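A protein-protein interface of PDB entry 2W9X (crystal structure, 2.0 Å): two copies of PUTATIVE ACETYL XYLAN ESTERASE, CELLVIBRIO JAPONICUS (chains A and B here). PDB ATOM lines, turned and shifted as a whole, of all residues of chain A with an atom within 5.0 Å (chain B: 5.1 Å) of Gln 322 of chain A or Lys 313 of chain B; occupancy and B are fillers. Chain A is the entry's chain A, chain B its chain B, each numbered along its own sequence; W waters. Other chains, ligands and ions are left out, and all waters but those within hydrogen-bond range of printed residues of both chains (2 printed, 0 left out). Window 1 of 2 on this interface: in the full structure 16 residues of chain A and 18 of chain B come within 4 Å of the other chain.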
ATOM      1  N   LEU A 291     -34.712 -18.253  28.412  1.00  0.00           N
ATOM      2  CA  LEU A 291     -34.859 -19.549  27.758  1.00  0.00           C
ATOM      3  C   LEU A 291     -33.634 -20.390  28.106  1.00  0.00           C
ATOM      4  O   LEU A 291     -32.543 -20.127  27.632  1.00  0.00           O
ATOM      5  CB  LEU A 291     -35.007 -19.389  26.231  1.00  0.00           C
ATOM      6  CG  LEU A 291     -36.081 -18.413  25.702  1.00  0.00           C
ATOM      7  CD1 LEU A 291     -36.404 -18.747  24.258  1.00  0.00           C
ATOM      8  CD2 LEU A 291     -37.326 -18.518  26.543  1.00  0.00           C
ATOM      9  N   ALA A 302     -29.638 -26.344  22.018  1.00  0.00           N
ATOM     10  CA  ALA A 302     -29.227 -24.956  22.208  1.00  0.00           C
ATOM     11  C   ALA A 302     -29.358 -24.155  20.932  1.00  0.00           C
ATOM     12  O   ALA A 302     -29.750 -22.980  20.979  1.00  0.00           O
ATOM     13  CB  ALA A 302     -27.795 -24.875  22.742  1.00  0.00           C
ATOM     14  N   VAL A 305     -32.996 -23.132  20.199  1.00  0.00           N
ATOM     15  CA  VAL A 305     -33.347 -22.022  21.103  1.00  0.00           C
ATOM     16  C   VAL A 305     -32.701 -20.676  20.690  1.00  0.00           C
ATOM     17  O   VAL A 305     -33.320 -19.619  20.820  1.00  0.00           O
ATOM     18  CB  VAL A 305     -33.060 -22.387  22.607  1.00  0.00           C
ATOM     19  CG1 VAL A 305     -33.265 -21.177  23.544  1.00  0.00           C
ATOM     20  CG2 VAL A 305     -33.991 -23.525  23.058  1.00  0.00           C
ATOM     21  N   GLY A 306     -31.464 -20.720  20.200  1.00  0.00           N
ATOM     22  CA  GLY A 306     -30.816 -19.537  19.597  1.00  0.00           C
ATOM     23  C   GLY A 306     -31.652 -18.922  18.487  1.00  0.00           C
ATOM     24  O   GLY A 306     -31.787 -17.688  18.401  1.00  0.00           O
ATOM     25  N   VAL A 309     -34.793 -17.224  20.055  1.00  0.00           N
ATOM     26  CA  VAL A 309     -34.441 -15.914  20.607  1.00  0.00           C
ATOM     27  C   VAL A 309     -34.269 -14.872  19.482  1.00  0.00           C
ATOM     28  O   VAL A 309     -34.805 -13.765  19.568  1.00  0.00           O
ATOM     29  CB  VAL A 309     -33.164 -15.987  21.498  1.00  0.00           C
ATOM     30  CG1 VAL A 309     -32.701 -14.577  21.897  1.00  0.00           C
ATOM     31  CG2 VAL A 309     -33.444 -16.811  22.743  1.00  0.00           C
ATOM     32  N   VAL A 320     -35.863 -11.049  26.026  1.00  0.00           N
ATOM     33  CA  VAL A 320     -35.678 -12.481  26.029  1.00  0.00           C
ATOM     34  C   VAL A 320     -34.173 -12.790  25.908  1.00  0.00           C
ATOM     35  O   VAL A 320     -33.446 -12.146  25.131  1.00  0.00           O
ATOM     36  CB  VAL A 320     -36.518 -13.179  24.921  1.00  0.00           C
ATOM     37  CG1 VAL A 320     -36.107 -12.710  23.520  1.00  0.00           C
ATOM     38  CG2 VAL A 320     -36.427 -14.710  25.056  1.00  0.00           C
ATOM     39  N   GLU A 321     -33.723 -13.742  26.724  1.00  0.00           N
ATOM     40  CA  GLU A 321     -32.323 -14.145  26.768  1.00  0.00           C
ATOM     41  C   GLU A 321     -32.225 -15.666  26.812  1.00  0.00           C
ATOM     42  O   GLU A 321     -33.172 -16.365  27.222  1.00  0.00           O
ATOM     43  CB  GLU A 321     -31.635 -13.614  28.024  1.00  0.00           C
ATOM     44  CG  GLU A 321     -31.714 -12.123  28.269  1.00  0.00           C
ATOM     45  CD  GLU A 321     -31.151 -11.767  29.639  1.00  0.00           C
ATOM     46  OE1 GLU A 321     -29.954 -11.411  29.718  1.00  0.00           O
ATOM     47  OE2 GLU A 321     -31.902 -11.889  30.637  1.00  0.00           O
ATOM     48  N   GLN A 322     -31.061 -16.164  26.410  1.00  0.00           N
ATOM     49  CA  GLN A 322     -30.755 -17.584  26.480  1.00  0.00           C
ATOM     50  C   GLN A 322     -29.756 -17.862  27.603  1.00  0.00           C
ATOM     51  O   GLN A 322     -28.853 -17.044  27.865  1.00  0.00           O
ATOM     52  CB  GLN A 322     -30.152 -18.042  25.142  1.00  0.00           C
ATOM     53  CG  GLN A 322     -29.750 -19.512  25.100  1.00  0.00           C
ATOM     54  CD  GLN A 322     -29.410 -19.956  23.696  1.00  0.00           C
ATOM     55  OE1 GLN A 322     -28.961 -19.154  22.874  1.00  0.00           O
ATOM     56  NE2 GLN A 322     -29.641 -21.240  23.407  1.00  0.00           N
ATOM     57  N   ILE A 323     -29.938 -19.010  28.257  1.00  0.00           N
ATOM     58  CA  ILE A 323     -28.946 -19.582  29.169  1.00  0.00           C
ATOM     59  C   ILE A 323     -28.732 -21.020  28.737  1.00  0.00           C
ATOM     60  O   ILE A 323     -29.693 -21.779  28.543  1.00  0.00           O
ATOM     61  CB  ILE A 323     -29.411 -19.536  30.659  1.00  0.00           C
ATOM     62  CG1 ILE A 323     -29.335 -18.103  31.190  1.00  0.00           C
ATOM     63  CG2 ILE A 323     -28.554 -20.504  31.550  1.00  0.00           C
ATOM     64  CD1 ILE A 323     -29.644 -17.948  32.689  1.00  0.00           C
ATOM     65  N   VAL A 324     -27.466 -21.379  28.539  1.00  0.00           N
ATOM     66  CA  VAL A 324     -27.103 -22.746  28.244  1.00  0.00           C
ATOM     67  C   VAL A 324     -26.305 -23.248  29.437  1.00  0.00           C
ATOM     68  O   VAL A 324     -25.240 -22.702  29.753  1.00  0.00           O
ATOM     69  CB  VAL A 324     -26.255 -22.902  26.949  1.00  0.00           C
ATOM     70  CG1 VAL A 324     -25.914 -24.384  26.739  1.00  0.00           C
ATOM     71  CG2 VAL A 324     -26.990 -22.344  25.709  1.00  0.00           C
ATOM     72  N   LYS A 326     -24.134 -26.022  31.788  1.00  0.00           N
ATOM     73  CA  LYS A 326     -23.029 -26.918  31.549  1.00  0.00           C
ATOM     74  C   LYS A 326     -22.510 -27.493  32.871  1.00  0.00           C
ATOM     75  O   LYS A 326     -22.666 -26.878  33.935  1.00  0.00           O
ATOM     76  CB  LYS A 326     -21.843 -26.168  30.884  1.00  0.00           C
ATOM     77  CG  LYS A 326     -22.138 -25.433  29.539  1.00  0.00           C
ATOM     78  CD  LYS A 326     -20.897 -24.693  29.057  1.00  0.00           C
ATOM     79  CE  LYS A 326     -19.756 -25.641  28.640  1.00  0.00           C
ATOM     80  NZ  LYS A 326     -20.283 -26.744  27.783  1.00  0.00           N
ATOM     81  N   GLY B 306     -28.186 -15.661  16.012  1.00  0.00           N
ATOM     82  CA  GLY B 306     -28.789 -16.487  17.074  1.00  0.00           C
ATOM     83  C   GLY B 306     -28.028 -17.795  17.288  1.00  0.00           C
ATOM     84  O   GLY B 306     -27.842 -18.253  18.438  1.00  0.00           O
ATOM     85  N   VAL B 308     -24.802 -18.244  16.483  1.00  0.00           N
ATOM     86  CA  VAL B 308     -23.513 -17.819  17.048  1.00  0.00           C
ATOM     87  C   VAL B 308     -23.594 -17.665  18.574  1.00  0.00           C
ATOM     88  O   VAL B 308     -22.769 -18.211  19.310  1.00  0.00           O
ATOM     89  CB  VAL B 308     -22.995 -16.509  16.392  1.00  0.00           C
ATOM     90  CG1 VAL B 308     -21.721 -15.985  17.082  1.00  0.00           C
ATOM     91  CG2 VAL B 308     -22.695 -16.747  14.918  1.00  0.00           C
ATOM     92  N   VAL B 309     -24.590 -16.932  19.052  1.00  0.00           N
ATOM     93  CA  VAL B 309     -24.751 -16.726  20.496  1.00  0.00           C
ATOM     94  C   VAL B 309     -24.928 -18.082  21.207  1.00  0.00           C
ATOM     95  O   VAL B 309     -24.321 -18.347  22.260  1.00  0.00           O
ATOM     96  CB  VAL B 309     -25.957 -15.800  20.814  1.00  0.00           C
ATOM     97  CG1 VAL B 309     -26.173 -15.720  22.330  1.00  0.00           C
ATOM     98  CG2 VAL B 309     -25.728 -14.420  20.238  1.00  0.00           C
ATOM     99  N   ALA B 310     -25.752 -18.944  20.618  1.00  0.00           N
ATOM    100  CA  ALA B 310     -25.999 -20.275  21.185  1.00  0.00           C
ATOM    101  C   ALA B 310     -24.764 -21.170  21.256  1.00  0.00           C
ATOM    102  O   ALA B 310     -24.562 -21.860  22.266  1.00  0.00           O
ATOM    103  CB  ALA B 310     -27.137 -20.973  20.432  1.00  0.00           C
ATOM    104  N   GLN B 311     -23.939 -21.123  20.213  1.00  0.00           N
ATOM    105  CA  GLN B 311     -22.713 -21.908  20.132  1.00  0.00           C
ATOM    106  C   GLN B 311     -21.619 -21.384  21.043  1.00  0.00           C
ATOM    107  O   GLN B 311     -20.790 -22.155  21.524  1.00  0.00           O
ATOM    108  CB  GLN B 311     -22.217 -21.979  18.688  1.00  0.00           C
ATOM    109  CG  GLN B 311     -22.809 -23.146  17.929  1.00  0.00           C
ATOM    110  CD  GLN B 311     -22.263 -23.290  16.537  1.00  0.00           C
ATOM    111  OE1 GLN B 311     -22.883 -23.911  15.677  1.00  0.00           O
ATOM    112  NE2 GLN B 311     -21.095 -22.725  16.303  1.00  0.00           N
ATOM    113  N   LEU B 312     -21.617 -20.071  21.261  1.00  0.00           N
ATOM    114  CA  LEU B 312     -20.737 -19.440  22.218  1.00  0.00           C
ATOM    115  C   LEU B 312     -21.089 -19.879  23.636  1.00  0.00           C
ATOM    116  O   LEU B 312     -20.216 -20.349  24.367  1.00  0.00           O
ATOM    117  CB  LEU B 312     -20.759 -17.908  22.091  1.00  0.00           C
ATOM    118  CG  LEU B 312     -19.933 -17.336  20.922  1.00  0.00           C
ATOM    119  CD1 LEU B 312     -20.421 -15.910  20.558  1.00  0.00           C
ATOM    120  CD2 LEU B 312     -18.419 -17.374  21.206  1.00  0.00           C
ATOM    121  N   LYS B 313     -22.361 -19.740  24.010  1.00  0.00           N
ATOM    122  CA  LYS B 313     -22.829 -20.140  25.346  1.00  0.00           C
ATOM    123  C   LYS B 313     -22.631 -21.634  25.597  1.00  0.00           C
ATOM    124  O   LYS B 313     -22.185 -22.031  26.664  1.00  0.00           O
ATOM    125  CB  LYS B 313     -24.297 -19.765  25.531  1.00  0.00           C
ATOM    126  CG  LYS B 313     -24.532 -18.288  25.609  1.00  0.00           C
ATOM    127  CD  LYS B 313     -26.013 -17.998  25.782  1.00  0.00           C
ATOM    128  CE  LYS B 313     -26.279 -16.510  25.951  1.00  0.00           C
ATOM    129  NZ  LYS B 313     -25.867 -16.051  27.311  1.00  0.00           N
ATOM    130  N   GLY B 314     -22.941 -22.447  24.587  1.00  0.00           N
ATOM    131  CA  GLY B 314     -22.737 -23.887  24.608  1.00  0.00           C
ATOM    132  C   GLY B 314     -21.294 -24.302  24.824  1.00  0.00           C
ATOM    133  O   GLY B 314     -21.026 -25.340  25.417  1.00  0.00           O
ATOM    134  N   GLY B 315     -20.369 -23.479  24.350  1.00  0.00           N
ATOM    135  CA  GLY B 315     -18.941 -23.699  24.578  1.00  0.00           C
ATOM    136  C   GLY B 315     -18.434 -23.114  25.891  1.00  0.00           C
ATOM    137  O   GLY B 315     -17.252 -23.267  26.232  1.00  0.00           O
ATOM    138  N   GLY B 316     -19.300 -22.435  26.634  1.00  0.00           N
ATOM    139  CA  GLY B 316     -18.898 -21.928  27.943  1.00  0.00           C
ATOM    140  C   GLY B 316     -18.599 -20.441  28.020  1.00  0.00           C
ATOM    141  O   GLY B 316     -18.133 -19.971  29.053  1.00  0.00           O
ATOM    142  N   LEU B 317     -18.855 -19.706  26.935  1.00  0.00           N
ATOM    143  CA  LEU B 317     -18.680 -18.259  26.912  1.00  0.00           C
ATOM    144  C   LEU B 317     -20.051 -17.611  27.028  1.00  0.00           C
ATOM    145  O   LEU B 317     -20.735 -17.375  26.025  1.00  0.00           O
ATOM    146  CB  LEU B 317     -17.981 -17.800  25.622  1.00  0.00           C
ATOM    147  CG  LEU B 317     -17.352 -16.390  25.608  1.00  0.00           C
ATOM    148  CD1 LEU B 317     -16.225 -16.348  24.584  1.00  0.00           C
ATOM    149  CD2 LEU B 317     -18.366 -15.281  25.326  1.00  0.00           C
ATOM    150  N   HIS B 318     -20.460 -17.334  28.254  1.00  0.00           N
ATOM    151  CA  HIS B 318     -21.831 -16.984  28.482  1.00  0.00           C
ATOM    152  C   HIS B 318     -22.095 -15.481  28.394  1.00  0.00           C
ATOM    153  O   HIS B 318     -23.238 -15.074  28.211  1.00  0.00           O
ATOM    154  CB  HIS B 318     -22.312 -17.582  29.804  1.00  0.00           C
ATOM    155  CG  HIS B 318     -22.056 -19.060  29.928  1.00  0.00           C
ATOM    156  ND1 HIS B 318     -22.754 -20.008  29.204  1.00  0.00           N
ATOM    157  CD2 HIS B 318     -21.190 -19.750  30.717  1.00  0.00           C
ATOM    158  CE1 HIS B 318     -22.326 -21.212  29.541  1.00  0.00           C
ATOM    159  NE2 HIS B 318     -21.379 -21.084  30.456  1.00  0.00           N
ATOM    160  N   VAL B 320     -22.449 -13.089  26.456  1.00  0.00           N
ATOM    161  CA  VAL B 320     -22.760 -12.651  25.114  1.00  0.00           C
ATOM    162  C   VAL B 320     -24.286 -12.556  24.967  1.00  0.00           C
ATOM    163  O   VAL B 320     -25.041 -13.388  25.494  1.00  0.00           O
ATOM    164  CB  VAL B 320     -22.039 -13.544  24.033  1.00  0.00           C
ATOM    165  CG1 VAL B 320     -22.404 -15.013  24.190  1.00  0.00           C
ATOM    166  CG2 VAL B 320     -22.278 -13.029  22.591  1.00  0.00           C
HETATM  167  O   HOH W   1     -25.497 -19.174  28.969  1.00  0.00           O
HETATM  168  O   HOH W   2     -24.466 -21.363  31.990  1.00  0.00           O
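The side-chain amino group (NZ) of Lys 326 of chain A lies within hydrogen-bond range of the backbone carbonyl oxygen (O) of Gly 314 of chain B (2.8 Å).
NZ of Lys 313 of chain B is in hydrogen-bond range of O of Gln 322 of chain A, at 3.2 Å.
The side-chain amino group of Lys 313 of chain B sits at hydrogen-bond distance from the backbone carbonyl oxygen of His 318 of chain B (2.9 Å).
The backbone carbonyl oxygen (O) of Ala 302 of chain A lies within hydrogen-bond range of the side-chain amide nitrogen (NE2) of Gln 322 of chain A.
The side-chain amino group (NZ) of Lys 313 of chain B lies within hydrogen-bond range of the backbone carbonyl oxygen (O) of Val 320 of chain B (3.3 Å).
O of Ala 302 of chain A touches CB of Ala 310 of chain B, at 3.3 Å.
Gly 306 of chain A touches Gly 306 of chain B (CA to O, 3.4 Å).
OE1 of Gln 322 of chain A touches CB of Ala 310 of chain B (3.5 Å).
Val 324 of chain A touches Lys 313 of chain B (CG2 to CB, 3.7 Å).
CG1 of Val 324 of chain A touches CA of Gly 314 of chain B, at 3.9 Å.
Val 324 of chain A touches His 318 of chain B (O to CE1, 3.3 Å).
Lys 326 of chain A touches Lys 313 of chain B.
Lys 326 of chain A touches Gly 315 of chain B.
Lys 326 of chain A touches Gly 316 of chain B (CD to CA, 3.6 Å).
Lys 326 of chain A touches His 318 of chain B.
Gln 322 of chain A touches two residues of chain B.
Printed residues of chain B within 4 Å of Ala 302 of chain A: Ala 310 (3.3 Å).
Of the printed residues of chain A, Gly 306 of chain B touches Gly 306.
Printed residues of chain A within 4 Å of Gly 315 of chain B: Lys 326 (3.96 Å).
Of the printed residues of chain B, Gly 306 of chain A touches Gly 306.
The nearest residue of chain A that does not touch Lys 313 of chain B is Ile 323 of chain A (4.7 Å).
Hydrophobic or aromatic side chains of chain B that line the printed part of chain A: Ala 310 and His 318.
Of the 11 printed residues of chain A, 5 touch a printed residue of chain B.
Hydrophobic or aromatic side chains of chain A within 4 Å of the printed part of chain B: Val 324.
Among the printed residues, 12 pairs touch across the chains.
Among the printed residues, no Asp or Glu carboxylate lies within 4 Å of a Lys or Arg side-chain nitrogen of the other chain.
Gly 306 of chain B touches its own counterpart, Gly 306 of chain A.
Of the 12 pairs that touch across the chains among the printed residues, 1 has its exchanged pair printed and touching as well.
Water W2 lies within hydrogen-bond range of O of Val 324 of chain A (2.7 Å) and NE2 of His 318 of chain B (3.5 Å).
Water W1 lies within hydrogen-bond range of a ring nitrogen (ND1) of His 318 of chain B (2.9 Å) and the backbone NH (N) of Val 324 of chain A (3.0 Å).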
